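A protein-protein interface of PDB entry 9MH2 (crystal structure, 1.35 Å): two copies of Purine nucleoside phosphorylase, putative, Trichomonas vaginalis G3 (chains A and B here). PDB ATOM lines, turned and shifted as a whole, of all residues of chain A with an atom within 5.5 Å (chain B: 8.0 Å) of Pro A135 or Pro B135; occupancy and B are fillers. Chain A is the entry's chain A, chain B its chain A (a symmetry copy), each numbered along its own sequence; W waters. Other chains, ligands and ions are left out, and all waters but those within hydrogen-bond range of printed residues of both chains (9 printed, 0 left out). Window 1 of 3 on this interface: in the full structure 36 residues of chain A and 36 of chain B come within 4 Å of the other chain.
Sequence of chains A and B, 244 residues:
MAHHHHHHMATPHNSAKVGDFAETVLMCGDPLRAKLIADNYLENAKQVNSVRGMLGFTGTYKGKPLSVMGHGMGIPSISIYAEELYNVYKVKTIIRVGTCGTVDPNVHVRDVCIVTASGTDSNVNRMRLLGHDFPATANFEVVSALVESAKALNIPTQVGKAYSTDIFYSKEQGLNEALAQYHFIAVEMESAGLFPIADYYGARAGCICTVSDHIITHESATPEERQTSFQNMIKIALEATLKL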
ATOM      1  N   ALA A 117      29.213  -3.456  14.355  1.00  0.00           N
ATOM      2  CA  ALA A 117      27.782  -3.277  14.569  1.00  0.00           C
ATOM      3  C   ALA A 117      27.629  -1.996  15.372  1.00  0.00           C
ATOM      4  O   ALA A 117      28.584  -1.534  15.991  1.00  0.00           O
ATOM      5  CB  ALA A 117      27.172  -4.451  15.339  1.00  0.00           C
ATOM      6  N   SER A 118      26.422  -1.429  15.368  1.00  0.00           N
ATOM      7  CA  SER A 118      26.171  -0.184  16.085  1.00  0.00           C
ATOM      8  C   SER A 118      24.860  -0.253  16.846  1.00  0.00           C
ATOM      9  O   SER A 118      23.831  -0.618  16.281  1.00  0.00           O
ATOM     10  CB  SER A 118      26.121   1.010  15.130  1.00  0.00           C
ATOM     11  OG  SER A 118      26.228   2.220  15.856  1.00  0.00           O
ATOM     12  N   GLY A 119      24.913   0.122  18.121  1.00  0.00           N
ATOM     13  CA  GLY A 119      23.711   0.297  18.910  1.00  0.00           C
ATOM     14  C   GLY A 119      23.139   1.675  18.666  1.00  0.00           C
ATOM     15  O   GLY A 119      23.705   2.487  17.936  1.00  0.00           O
ATOM     16  N   THR A 120      22.013   1.963  19.314  1.00  0.00           N
ATOM     17  CA  THR A 120      21.364   3.250  19.096  1.00  0.00           C
ATOM     18  C   THR A 120      20.302   3.498  20.148  1.00  0.00           C
ATOM     19  O   THR A 120      19.797   2.571  20.778  1.00  0.00           O
ATOM     20  CB  THR A 120      20.762   3.336  17.683  1.00  0.00           C
ATOM     21  OG1 THR A 120      20.257   4.654  17.453  1.00  0.00           O
ATOM     22  CG2 THR A 120      19.638   2.354  17.477  1.00  0.00           C
ATOM     23  N   ASP A 133      14.737  -6.321  19.116  1.00  0.00           N
ATOM     24  CA  ASP A 133      16.115  -5.872  18.957  1.00  0.00           C
ATOM     25  C   ASP A 133      16.643  -6.366  17.619  1.00  0.00           C
ATOM     26  O   ASP A 133      16.830  -7.570  17.424  1.00  0.00           O
ATOM     27  CB  ASP A 133      17.021  -6.416  20.058  1.00  0.00           C
ATOM     28  CG  ASP A 133      16.853  -5.704  21.386  1.00  0.00           C
ATOM     29  OD1 ASP A 133      15.897  -4.921  21.533  1.00  0.00           O
ATOM     30  OD2 ASP A 133      17.705  -5.914  22.285  1.00  0.00           O
ATOM     31  N   PHE A 134      16.945  -5.426  16.740  1.00  0.00           N
ATOM     32  CA  PHE A 134      17.500  -5.667  15.416  1.00  0.00           C
ATOM     33  C   PHE A 134      18.913  -5.099  15.427  1.00  0.00           C
ATOM     34  O   PHE A 134      19.079  -3.873  15.437  1.00  0.00           O
ATOM     35  CB  PHE A 134      16.606  -4.905  14.432  1.00  0.00           C
ATOM     36  CG  PHE A 134      17.004  -5.011  12.971  1.00  0.00           C
ATOM     37  CD1 PHE A 134      18.243  -5.461  12.547  1.00  0.00           C
ATOM     38  CD2 PHE A 134      16.092  -4.612  12.016  1.00  0.00           C
ATOM     39  CE1 PHE A 134      18.550  -5.483  11.186  1.00  0.00           C
ATOM     40  CE2 PHE A 134      16.385  -4.656  10.681  1.00  0.00           C
ATOM     41  CZ  PHE A 134      17.616  -5.087  10.261  1.00  0.00           C
ATOM     42  N   PRO A 135      19.964  -5.918  15.407  1.00  0.00           N
ATOM     43  CA  PRO A 135      21.321  -5.353  15.450  1.00  0.00           C
ATOM     44  C   PRO A 135      21.683  -4.742  14.107  1.00  0.00           C
ATOM     45  O   PRO A 135      21.605  -5.404  13.071  1.00  0.00           O
ATOM     46  CB  PRO A 135      22.197  -6.570  15.756  1.00  0.00           C
ATOM     47  CG  PRO A 135      21.452  -7.713  15.124  1.00  0.00           C
ATOM     48  CD  PRO A 135      19.981  -7.386  15.317  1.00  0.00           C
ATOM     49  N   ALA A 136      22.049  -3.468  14.129  1.00  0.00           N
ATOM     50  CA  ALA A 136      22.601  -2.820  12.950  1.00  0.00           C
ATOM     51  C   ALA A 136      24.015  -3.354  12.755  1.00  0.00           C
ATOM     52  O   ALA A 136      24.919  -3.017  13.523  1.00  0.00           O
ATOM     53  CB  ALA A 136      22.591  -1.308  13.158  1.00  0.00           C
ATOM     54  N   THR A 137      24.206  -4.202  11.744  1.00  0.00           N
ATOM     55  CA  THR A 137      25.405  -5.018  11.595  1.00  0.00           C
ATOM     56  C   THR A 137      26.070  -4.731  10.254  1.00  0.00           C
ATOM     57  O   THR A 137      25.419  -4.766   9.206  1.00  0.00           O
ATOM     58  CB  THR A 137      25.028  -6.505  11.712  1.00  0.00           C
ATOM     59  OG1 THR A 137      24.223  -6.693  12.884  1.00  0.00           O
ATOM     60  CG2 THR A 137      26.265  -7.378  11.802  1.00  0.00           C
ATOM     61  N   LYS A 161      32.201  -2.380  18.339  1.00  0.00           N
ATOM     62  CA  LYS A 161      30.874  -1.774  18.295  1.00  0.00           C
ATOM     63  C   LYS A 161      30.926  -0.258  18.339  1.00  0.00           C
ATOM     64  O   LYS A 161      31.697   0.331  19.098  1.00  0.00           O
ATOM     65  CB  LYS A 161      30.046  -2.222  19.501  1.00  0.00           C
ATOM     66  CG  LYS A 161      29.827  -3.716  19.580  1.00  0.00           C
ATOM     67  CD  LYS A 161      28.926  -4.086  20.765  1.00  0.00           C
ATOM     68  CE  LYS A 161      29.520  -3.696  22.119  1.00  0.00           C
ATOM     69  NZ  LYS A 161      30.787  -4.395  22.436  1.00  0.00           N
ATOM     70  N   ALA A 162      30.042   0.363  17.568  1.00  0.00           N
ATOM     71  CA  ALA A 162      29.720   1.778  17.700  1.00  0.00           C
ATOM     72  C   ALA A 162      28.382   1.955  18.419  1.00  0.00           C
ATOM     73  O   ALA A 162      27.615   1.012  18.618  1.00  0.00           O
ATOM     74  CB  ALA A 162      29.670   2.450  16.325  1.00  0.00           C
ATOM     75  N   PHE A 184      32.035  -0.468  23.926  1.00  0.00           N
ATOM     76  CA  PHE A 184      31.744   0.290  22.718  1.00  0.00           C
ATOM     77  C   PHE A 184      32.935   1.193  22.424  1.00  0.00           C
ATOM     78  O   PHE A 184      33.413   1.913  23.309  1.00  0.00           O
ATOM     79  CB  PHE A 184      30.476   1.122  22.908  1.00  0.00           C
ATOM     80  CG  PHE A 184      29.205   0.310  22.862  1.00  0.00           C
ATOM     81  CD1 PHE A 184      28.766  -0.403  23.970  1.00  0.00           C
ATOM     82  CD2 PHE A 184      28.455   0.257  21.705  1.00  0.00           C
ATOM     83  CE1 PHE A 184      27.586  -1.135  23.916  1.00  0.00           C
ATOM     84  CE2 PHE A 184      27.291  -0.471  21.641  1.00  0.00           C
ATOM     85  CZ  PHE A 184      26.854  -1.173  22.747  1.00  0.00           C
ATOM     86  N   PRO A 196      20.804  -1.359   8.491  1.00  0.00           N
ATOM     87  CA  PRO A 196      19.544  -2.058   8.173  1.00  0.00           C
ATOM     88  C   PRO A 196      18.980  -1.711   6.808  1.00  0.00           C
ATOM     89  O   PRO A 196      18.299  -2.557   6.211  1.00  0.00           O
ATOM     90  CB  PRO A 196      18.603  -1.646   9.313  1.00  0.00           C
ATOM     91  CG  PRO A 196      19.540  -1.236  10.426  1.00  0.00           C
ATOM     92  CD  PRO A 196      20.674  -0.555   9.716  1.00  0.00           C
ATOM     93  N   ASP A 199      20.649  -3.959   4.468  1.00  0.00           N
ATOM     94  CA  ASP A 199      20.010  -5.271   4.574  1.00  0.00           C
ATOM     95  C   ASP A 199      18.739  -5.330   3.736  1.00  0.00           C
ATOM     96  O   ASP A 199      18.505  -6.302   3.008  1.00  0.00           O
ATOM     97  CB  ASP A 199      19.652  -5.597   6.023  1.00  0.00           C
ATOM     98  CG  ASP A 199      20.845  -5.893   6.888  1.00  0.00           C
ATOM     99  OD1 ASP A 199      21.909  -6.269   6.352  1.00  0.00           O
ATOM    100  OD2 ASP A 199      20.693  -5.784   8.131  1.00  0.00           O
ATOM    101  N   THR B 116      27.541 -13.025  12.789  1.00  0.00           N
ATOM    102  CA  THR B 116      28.238 -11.778  13.086  1.00  0.00           C
ATOM    103  C   THR B 116      27.568 -10.987  14.207  1.00  0.00           C
ATOM    104  O   THR B 116      28.249 -10.276  14.950  1.00  0.00           O
ATOM    105  CB  THR B 116      28.285 -10.901  11.835  1.00  0.00           C
ATOM    106  OG1 THR B 116      26.966 -10.803  11.294  1.00  0.00           O
ATOM    107  CG2 THR B 116      29.243 -11.488  10.797  1.00  0.00           C
ATOM    108  N   ALA B 117      26.249 -11.086  14.339  1.00  0.00           N
ATOM    109  CA  ALA B 117      25.504 -10.422  15.402  1.00  0.00           C
ATOM    110  C   ALA B 117      24.158 -11.122  15.479  1.00  0.00           C
ATOM    111  O   ALA B 117      23.755 -11.799  14.535  1.00  0.00           O
ATOM    112  CB  ALA B 117      25.301  -8.934  15.109  1.00  0.00           C
ATOM    113  N   SER B 118      23.459 -10.951  16.601  1.00  0.00           N
ATOM    114  CA  SER B 118      22.165 -11.598  16.790  1.00  0.00           C
ATOM    115  C   SER B 118      21.159 -10.633  17.388  1.00  0.00           C
ATOM    116  O   SER B 118      21.444  -9.979  18.391  1.00  0.00           O
ATOM    117  CB  SER B 118      22.279 -12.817  17.708  1.00  0.00           C
ATOM    118  OG  SER B 118      21.118 -13.619  17.600  1.00  0.00           O
ATOM    119  N   GLY B 119      19.981 -10.571  16.774  1.00  0.00           N
ATOM    120  CA  GLY B 119      18.864  -9.849  17.346  1.00  0.00           C
ATOM    121  C   GLY B 119      18.149 -10.728  18.345  1.00  0.00           C
ATOM    122  O   GLY B 119      18.492 -11.892  18.541  1.00  0.00           O
ATOM    123  N   THR B 120      17.109 -10.178  18.968  1.00  0.00           N
ATOM    124  CA  THR B 120      16.393 -10.936  19.987  1.00  0.00           C
ATOM    125  C   THR B 120      15.080 -10.264  20.329  1.00  0.00           C
ATOM    126  O   THR B 120      14.894  -9.069  20.104  1.00  0.00           O
ATOM    127  CB  THR B 120      17.255 -11.123  21.248  1.00  0.00           C
ATOM    128  OG1 THR B 120      16.582 -11.985  22.169  1.00  0.00           O
ATOM    129  CG2 THR B 120      17.545  -9.817  21.943  1.00  0.00           C
ATOM    130  N   ASN B 125      19.311  -7.301  26.945  1.00  0.00           N
ATOM    131  CA  ASN B 125      20.301  -6.342  26.469  1.00  0.00           C
ATOM    132  C   ASN B 125      19.833  -4.906  26.635  1.00  0.00           C
ATOM    133  O   ASN B 125      20.647  -4.032  26.948  1.00  0.00           O
ATOM    134  CB  ASN B 125      20.704  -6.681  25.036  1.00  0.00           C
ATOM    135  CG  ASN B 125      21.385  -8.047  24.968  1.00  0.00           C
ATOM    136  OD1 ASN B 125      21.987  -8.479  25.944  1.00  0.00           O
ATOM    137  ND2 ASN B 125      21.272  -8.733  23.837  1.00  0.00           N
ATOM    138  N   LEU B 129      21.836  -1.510  28.740  1.00  0.00           N
ATOM    139  CA  LEU B 129      22.195  -0.263  28.065  1.00  0.00           C
ATOM    140  C   LEU B 129      21.085   0.763  28.196  1.00  0.00           C
ATOM    141  O   LEU B 129      20.694   1.425  27.235  1.00  0.00           O
ATOM    142  CB  LEU B 129      22.578  -0.523  26.611  1.00  0.00           C
ATOM    143  CG  LEU B 129      23.470   0.542  25.972  1.00  0.00           C
ATOM    144  CD1 LEU B 129      24.819   0.581  26.679  1.00  0.00           C
ATOM    145  CD2 LEU B 129      23.664   0.253  24.483  1.00  0.00           C
ATOM    146  N   HIS B 132      18.175   1.025  25.713  1.00  0.00           N
ATOM    147  CA  HIS B 132      18.420   1.303  24.306  1.00  0.00           C
ATOM    148  C   HIS B 132      18.739   0.014  23.554  1.00  0.00           C
ATOM    149  O   HIS B 132      18.665  -1.086  24.112  1.00  0.00           O
ATOM    150  CB  HIS B 132      19.536   2.330  24.173  1.00  0.00           C
ATOM    151  CG  HIS B 132      19.287   3.578  24.946  1.00  0.00           C
ATOM    152  ND1 HIS B 132      18.123   4.307  24.825  1.00  0.00           N
ATOM    153  CD2 HIS B 132      20.051   4.231  25.852  1.00  0.00           C
ATOM    154  CE1 HIS B 132      18.184   5.359  25.622  1.00  0.00           C
ATOM    155  NE2 HIS B 132      19.346   5.338  26.252  1.00  0.00           N
ATOM    156  N   ASP B 133      19.095   0.155  22.270  1.00  0.00           N
ATOM    157  CA  ASP B 133      19.454  -0.967  21.410  1.00  0.00           C
ATOM    158  C   ASP B 133      20.939  -1.253  21.566  1.00  0.00           C
ATOM    159  O   ASP B 133      21.780  -0.446  21.159  1.00  0.00           O
ATOM    160  CB  ASP B 133      19.178  -0.667  19.939  1.00  0.00           C
ATOM    161  CG  ASP B 133      17.709  -0.745  19.572  1.00  0.00           C
ATOM    162  OD1 ASP B 133      16.864  -0.830  20.482  1.00  0.00           O
ATOM    163  OD2 ASP B 133      17.400  -0.745  18.355  1.00  0.00           O
ATOM    164  N   PHE B 134      21.245  -2.428  22.089  1.00  0.00           N
ATOM    165  CA  PHE B 134      22.597  -2.925  22.294  1.00  0.00           C
ATOM    166  C   PHE B 134      22.772  -4.108  21.350  1.00  0.00           C
ATOM    167  O   PHE B 134      22.186  -5.171  21.588  1.00  0.00           O
ATOM    168  CB  PHE B 134      22.673  -3.371  23.758  1.00  0.00           C
ATOM    169  CG  PHE B 134      24.009  -3.936  24.201  1.00  0.00           C
ATOM    170  CD1 PHE B 134      24.996  -4.347  23.320  1.00  0.00           C
ATOM    171  CD2 PHE B 134      24.244  -4.073  25.554  1.00  0.00           C
ATOM    172  CE1 PHE B 134      26.180  -4.903  23.805  1.00  0.00           C
ATOM    173  CE2 PHE B 134      25.415  -4.596  26.029  1.00  0.00           C
ATOM    174  CZ  PHE B 134      26.385  -5.017  25.158  1.00  0.00           C
ATOM    175  N   PRO B 135      23.569  -4.004  20.287  1.00  0.00           N
ATOM    176  CA  PRO B 135      23.701  -5.146  19.370  1.00  0.00           C
ATOM    177  C   PRO B 135      24.562  -6.231  19.995  1.00  0.00           C
ATOM    178  O   PRO B 135      25.693  -5.976  20.414  1.00  0.00           O
ATOM    179  CB  PRO B 135      24.388  -4.535  18.147  1.00  0.00           C
ATOM    180  CG  PRO B 135      25.225  -3.427  18.725  1.00  0.00           C
ATOM    181  CD  PRO B 135      24.406  -2.867  19.876  1.00  0.00           C
ATOM    182  N   ALA B 136      24.008  -7.432  20.084  1.00  0.00           N
ATOM    183  CA  ALA B 136      24.785  -8.595  20.483  1.00  0.00           C
ATOM    184  C   ALA B 136      25.694  -8.960  19.315  1.00  0.00           C
ATOM    185  O   ALA B 136      25.222  -9.464  18.293  1.00  0.00           O
ATOM    186  CB  ALA B 136      23.835  -9.735  20.839  1.00  0.00           C
ATOM    187  N   THR B 137      26.992  -8.689  19.452  1.00  0.00           N
ATOM    188  CA  THR B 137      27.938  -8.703  18.342  1.00  0.00           C
ATOM    189  C   THR B 137      29.067  -9.685  18.631  1.00  0.00           C
ATOM    190  O   THR B 137      29.688  -9.638  19.697  1.00  0.00           O
ATOM    191  CB  THR B 137      28.489  -7.284  18.124  1.00  0.00           C
ATOM    192  OG1 THR B 137      27.394  -6.359  18.067  1.00  0.00           O
ATOM    193  CG2 THR B 137      29.290  -7.199  16.838  1.00  0.00           C
ATOM    194  N   ALA B 138      29.337 -10.558  17.672  1.00  0.00           N
ATOM    195  CA  ALA B 138      30.445 -11.491  17.806  1.00  0.00           C
ATOM    196  C   ALA B 138      31.773 -10.754  17.673  1.00  0.00           C
ATOM    197  O   ALA B 138      31.880  -9.716  17.006  1.00  0.00           O
ATOM    198  CB  ALA B 138      30.360 -12.572  16.732  1.00  0.00           C
ATOM    199  N   GLY B 160      26.435 -13.892   8.582  1.00  0.00           N
ATOM    200  CA  GLY B 160      25.457 -12.836   8.778  1.00  0.00           C
ATOM    201  C   GLY B 160      24.740 -12.935  10.116  1.00  0.00           C
ATOM    202  O   GLY B 160      25.225 -13.569  11.059  1.00  0.00           O
ATOM    203  N   LYS B 161      23.573 -12.283  10.171  1.00  0.00           N
ATOM    204  CA  LYS B 161      22.845 -12.093  11.422  1.00  0.00           C
ATOM    205  C   LYS B 161      22.043 -13.318  11.818  1.00  0.00           C
ATOM    206  O   LYS B 161      21.402 -13.958  10.982  1.00  0.00           O
ATOM    207  CB  LYS B 161      21.850 -10.939  11.285  1.00  0.00           C
ATOM    208  CG  LYS B 161      22.488  -9.607  10.960  1.00  0.00           C
ATOM    209  CD  LYS B 161      21.444  -8.484  10.917  1.00  0.00           C
ATOM    210  CE  LYS B 161      20.379  -8.692   9.839  1.00  0.00           C
ATOM    211  NZ  LYS B 161      20.922  -8.693   8.461  1.00  0.00           N
ATOM    212  N   ALA B 162      22.027 -13.591  13.117  1.00  0.00           N
ATOM    213  CA  ALA B 162      21.081 -14.514  13.729  1.00  0.00           C
ATOM    214  C   ALA B 162      19.972 -13.744  14.446  1.00  0.00           C
ATOM    215  O   ALA B 162      20.045 -12.533  14.654  1.00  0.00           O
ATOM    216  CB  ALA B 162      21.795 -15.444  14.714  1.00  0.00           C
ATOM    217  N   TYR B 163      18.930 -14.479  14.829  1.00  0.00           N
ATOM    218  CA  TYR B 163      17.864 -13.975  15.684  1.00  0.00           C
ATOM    219  C   TYR B 163      17.668 -15.000  16.789  1.00  0.00           C
ATOM    220  O   TYR B 163      17.348 -16.158  16.508  1.00  0.00           O
ATOM    221  CB  TYR B 163      16.578 -13.789  14.887  1.00  0.00           C
ATOM    222  CG  TYR B 163      15.456 -13.120  15.648  1.00  0.00           C
ATOM    223  CD1 TYR B 163      15.497 -11.763  15.925  1.00  0.00           C
ATOM    224  CD2 TYR B 163      14.349 -13.831  16.077  1.00  0.00           C
ATOM    225  CE1 TYR B 163      14.487 -11.140  16.598  1.00  0.00           C
ATOM    226  CE2 TYR B 163      13.301 -13.200  16.763  1.00  0.00           C
ATOM    227  CZ  TYR B 163      13.391 -11.842  17.014  1.00  0.00           C
ATOM    228  OH  TYR B 163      12.407 -11.147  17.678  1.00  0.00           O
ATOM    229  N   SER B 164      17.878 -14.570  18.033  1.00  0.00           N
ATOM    230  CA  SER B 164      17.727 -15.400  19.222  1.00  0.00           C
ATOM    231  C   SER B 164      16.370 -15.108  19.856  1.00  0.00           C
ATOM    232  O   SER B 164      16.171 -14.041  20.441  1.00  0.00           O
ATOM    233  CB  SER B 164      18.846 -15.088  20.213  1.00  0.00           C
ATOM    234  OG  SER B 164      20.130 -15.238  19.634  1.00  0.00           O
ATOM    235  N   TYR B 182      15.116  -8.633   5.982  1.00  0.00           N
ATOM    236  CA  TYR B 182      16.398  -8.076   6.380  1.00  0.00           C
ATOM    237  C   TYR B 182      17.510  -9.112   6.383  1.00  0.00           C
ATOM    238  O   TYR B 182      18.605  -8.839   6.884  1.00  0.00           O
ATOM    239  CB  TYR B 182      16.265  -7.348   7.711  1.00  0.00           C
ATOM    240  CG  TYR B 182      15.373  -6.129   7.550  1.00  0.00           C
ATOM    241  CD1 TYR B 182      15.897  -4.919   7.114  1.00  0.00           C
ATOM    242  CD2 TYR B 182      14.000  -6.200   7.774  1.00  0.00           C
ATOM    243  CE1 TYR B 182      15.093  -3.813   6.941  1.00  0.00           C
ATOM    244  CE2 TYR B 182      13.181  -5.087   7.612  1.00  0.00           C
ATOM    245  CZ  TYR B 182      13.745  -3.896   7.183  1.00  0.00           C
ATOM    246  OH  TYR B 182      12.976  -2.772   7.001  1.00  0.00           O
ATOM    247  N   PHE B 184      18.139 -12.026   7.871  1.00  0.00           N
ATOM    248  CA  PHE B 184      18.595 -12.848   8.982  1.00  0.00           C
ATOM    249  C   PHE B 184      18.762 -14.277   8.479  1.00  0.00           C
ATOM    250  O   PHE B 184      17.855 -14.831   7.846  1.00  0.00           O
ATOM    251  CB  PHE B 184      17.587 -12.799  10.128  1.00  0.00           C
ATOM    252  CG  PHE B 184      17.613 -11.505  10.904  1.00  0.00           C
ATOM    253  CD1 PHE B 184      16.964 -10.370  10.435  1.00  0.00           C
ATOM    254  CD2 PHE B 184      18.296 -11.426  12.101  1.00  0.00           C
ATOM    255  CE1 PHE B 184      16.987  -9.190  11.168  1.00  0.00           C
ATOM    256  CE2 PHE B 184      18.329 -10.260  12.828  1.00  0.00           C
ATOM    257  CZ  PHE B 184      17.676  -9.136  12.361  1.00  0.00           C
ATOM    258  N   ALA B 192      22.285 -14.192  21.287  1.00  0.00           N
ATOM    259  CA  ALA B 192      22.118 -12.806  21.715  1.00  0.00           C
ATOM    260  C   ALA B 192      22.387 -12.627  23.200  1.00  0.00           C
ATOM    261  O   ALA B 192      22.663 -11.513  23.638  1.00  0.00           O
ATOM    262  CB  ALA B 192      20.730 -12.276  21.350  1.00  0.00           C
ATOM    263  N   PHE B 195      26.912 -12.895  23.599  1.00  0.00           N
ATOM    264  CA  PHE B 195      27.857 -11.874  23.159  1.00  0.00           C
ATOM    265  C   PHE B 195      27.993 -10.719  24.150  1.00  0.00           C
ATOM    266  O   PHE B 195      29.132 -10.282  24.397  1.00  0.00           O
ATOM    267  CB  PHE B 195      27.480 -11.375  21.755  1.00  0.00           C
ATOM    268  CG  PHE B 195      27.474 -12.461  20.687  1.00  0.00           C
ATOM    269  CD1 PHE B 195      28.238 -13.615  20.804  1.00  0.00           C
ATOM    270  CD2 PHE B 195      26.687 -12.313  19.558  1.00  0.00           C
ATOM    271  CE1 PHE B 195      28.226 -14.586  19.799  1.00  0.00           C
ATOM    272  CE2 PHE B 195      26.664 -13.270  18.566  1.00  0.00           C
ATOM    273  CZ  PHE B 195      27.442 -14.408  18.678  1.00  0.00           C
ATOM    274  N   PRO B 196      26.922 -10.188  24.743  1.00  0.00           N
ATOM    275  CA  PRO B 196      27.107  -9.072  25.691  1.00  0.00           C
ATOM    276  C   PRO B 196      27.808  -9.473  26.975  1.00  0.00           C
ATOM    277  O   PRO B 196      28.485  -8.624  27.575  1.00  0.00           O
ATOM    278  CB  PRO B 196      25.680  -8.567  25.940  1.00  0.00           C
ATOM    279  CG  PRO B 196      24.910  -9.042  24.729  1.00  0.00           C
ATOM    280  CD  PRO B 196      25.499 -10.390  24.428  1.00  0.00           C
ATOM    281  N   ASP B 199      31.376  -9.252  26.242  1.00  0.00           N
ATOM    282  CA  ASP B 199      31.757  -7.840  26.288  1.00  0.00           C
ATOM    283  C   ASP B 199      32.016  -7.389  27.720  1.00  0.00           C
ATOM    284  O   ASP B 199      33.012  -6.713  28.001  1.00  0.00           O
ATOM    285  CB  ASP B 199      30.667  -6.953  25.689  1.00  0.00           C
ATOM    286  CG  ASP B 199      30.545  -7.072  24.196  1.00  0.00           C
ATOM    287  OD1 ASP B 199      31.520  -7.486  23.534  1.00  0.00           O
ATOM    288  OD2 ASP B 199      29.460  -6.702  23.678  1.00  0.00           O
HETATM  289  O   HOH W   1      19.254  -1.331  16.378  1.00  0.00           O
HETATM  290  O   HOH W   2      19.202  -3.856  23.425  1.00  0.00           O
HETATM  291  O   HOH W   3      15.944  -2.819  17.190  1.00  0.00           O
HETATM  292  O   HOH W   4      20.189  -7.007  21.716  1.00  0.00           O
HETATM  293  O   HOH W   5      13.753  -7.122  22.504  1.00  0.00           O
HETATM  294  O   HOH W   6      17.287  -6.813  24.884  1.00  0.00           O
HETATM  295  O   HOH W   7      30.891  -7.416  20.884  1.00  0.00           O
HETATM  296  O   HOH W   8      16.516   2.335  20.973  1.00  0.00           O
HETATM  297  O   HOH W   9      23.741  -6.804   8.297  1.00  0.00           O
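The backbone NH (N) of Gly A119 is in hydrogen-bond range of the backbone carbonyl oxygen (O) of Ala A162, 2.9 Å away. The backbone carbonyl oxygen of Ser B164 is in hydrogen-bond range of the side-chain hydroxyl of Thr B120, at 2.7 Å. The backbone carbonyl oxygen (O) of Gly B119 is in hydrogen-bond range of the backbone NH (N) of Ser B164 (2.8 Å).
Ala A117 touches Thr B137, and with the chains exchanged Thr A137 touches Ala B117. Gly A119 touches Pro B135, and with the chains exchanged Pro A135 touches Gly B119. Thr A120 touches Asp B133, and with the chains exchanged Asp A133 touches Thr B120. Lys A161 touches Asp B199, and with the chains exchanged Asp A199 touches Lys B161. Positions printed for both chains: 117, 118, 119, 120, 133, 134, 135, 136, 137, 161, 162, 184, 196 and 199.
Water W4 lies within hydrogen-bond range of O of Phe B134 (2.7 Å), OD2 of Asp A133 (2.8 Å) and ND2 of Asn B125 (2.9 Å). Water W7 lies within hydrogen-bond range of OD1 of Asp B199, O of Thr B137 and NZ of Lys A161. Water W2 lies within hydrogen-bond range of OD2 of Asp A133, N of Phe B134 and O of His B132. Water W8 lies within hydrogen-bond range of OD1 of Asp B133 (3.2 Å) and O of Thr A120 (3.3 Å).
O of Thr A120 is in hydrogen-bond range of N of Asp B133. The backbone carbonyl oxygen of Thr B120 sits at hydrogen-bond distance from the backbone NH of Asp A133 (2.9 Å). OD2 of Asp A199 is in salt-bridge range of NZ of Lys B161 (2.9 Å). NZ of Lys A161 lies within salt-bridge range of OD2 of Asp B199, 2.9 Å away.
No residue of chain B comes within 4 Å of Ala A136. Of the printed residues of chain B, Pro A196 touches Tyr B182. Of the printed residues of chain A, Gly B119 touches Asp A133 (3.1 Å) and Pro A135 (3.4 Å). Printed residues of chain A within 4 Å of Pro B135: Ala A117, Ser A118, Gly A119, Pro A135 and Lys A161. Tyr B163 touches none of the printed residues of chain A. Ala B192 touches none of the printed residues of chain A. The nearest printed residue of chain A that does not touch Pro B135 is Phe A184 (4.1 Å).
Hydrophobic or aromatic side chains of chain A within 4 Å of the printed part of chain B: Ala A117, Phe A134, Pro A135 and Phe A184. Hydrophobic or aromatic side chains of chain B that line the printed part of chain A: Ala B117, Leu B129, His B132, Phe B134, Pro B135, Tyr B182 and Phe B184. Among the printed residues, Asp or Glu carboxylates within 4 Å of a Lys or Arg side-chain nitrogen of the other chain: Lys A161 with Asp B199 (2.9 Å) and Asp A199 with Lys B161 (2.9 Å).
Among the printed residues, merely in contact across the chains: Asp A133 with Gly B119 (3.1 Å), Gly A119 with Asp B133 (3.1 Å), Ala A117 with Thr B137 (3.3 Å), Thr A137 with Ala B117 (3.3 Å), Gly A119 with Pro B135 (3.4 Å), Pro A135 with Gly B119 (3.4 Å), Thr A120 with His B132 (3.4 Å), Pro A196 with Tyr B182 (3.5 Å), Asp A199 with Tyr B182 (3.5 Å), Thr A137 with Thr B116 (3.5 Å), Phe A134 with Tyr B182 (3.6 Å), Pro A135 with Ser B118 (3.7 Å), Ser A118 with Pro B135 (3.7 Å), Phe A184 with Phe B134 (3.7 Å), Phe A134 with Phe B184 (3.7 Å), Lys A161 with Pro B135 (3.8 Å), Pro A135 with Lys B161 (3.8 Å), Pro A135 with Pro B135 (3.8 Å), Lys A161 with Thr B137 (3.8 Å), Thr A137 with Lys B161 (3.8 Å), Phe A184 with Leu B129 (3.9 Å), Lys A161 with Phe B134 (3.9 Å), Phe A134 with Lys B161 (3.9 Å), Pro A135 with Ala B117 (3.95 Å) and Ala A117 with Pro B135 (3.96 Å).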
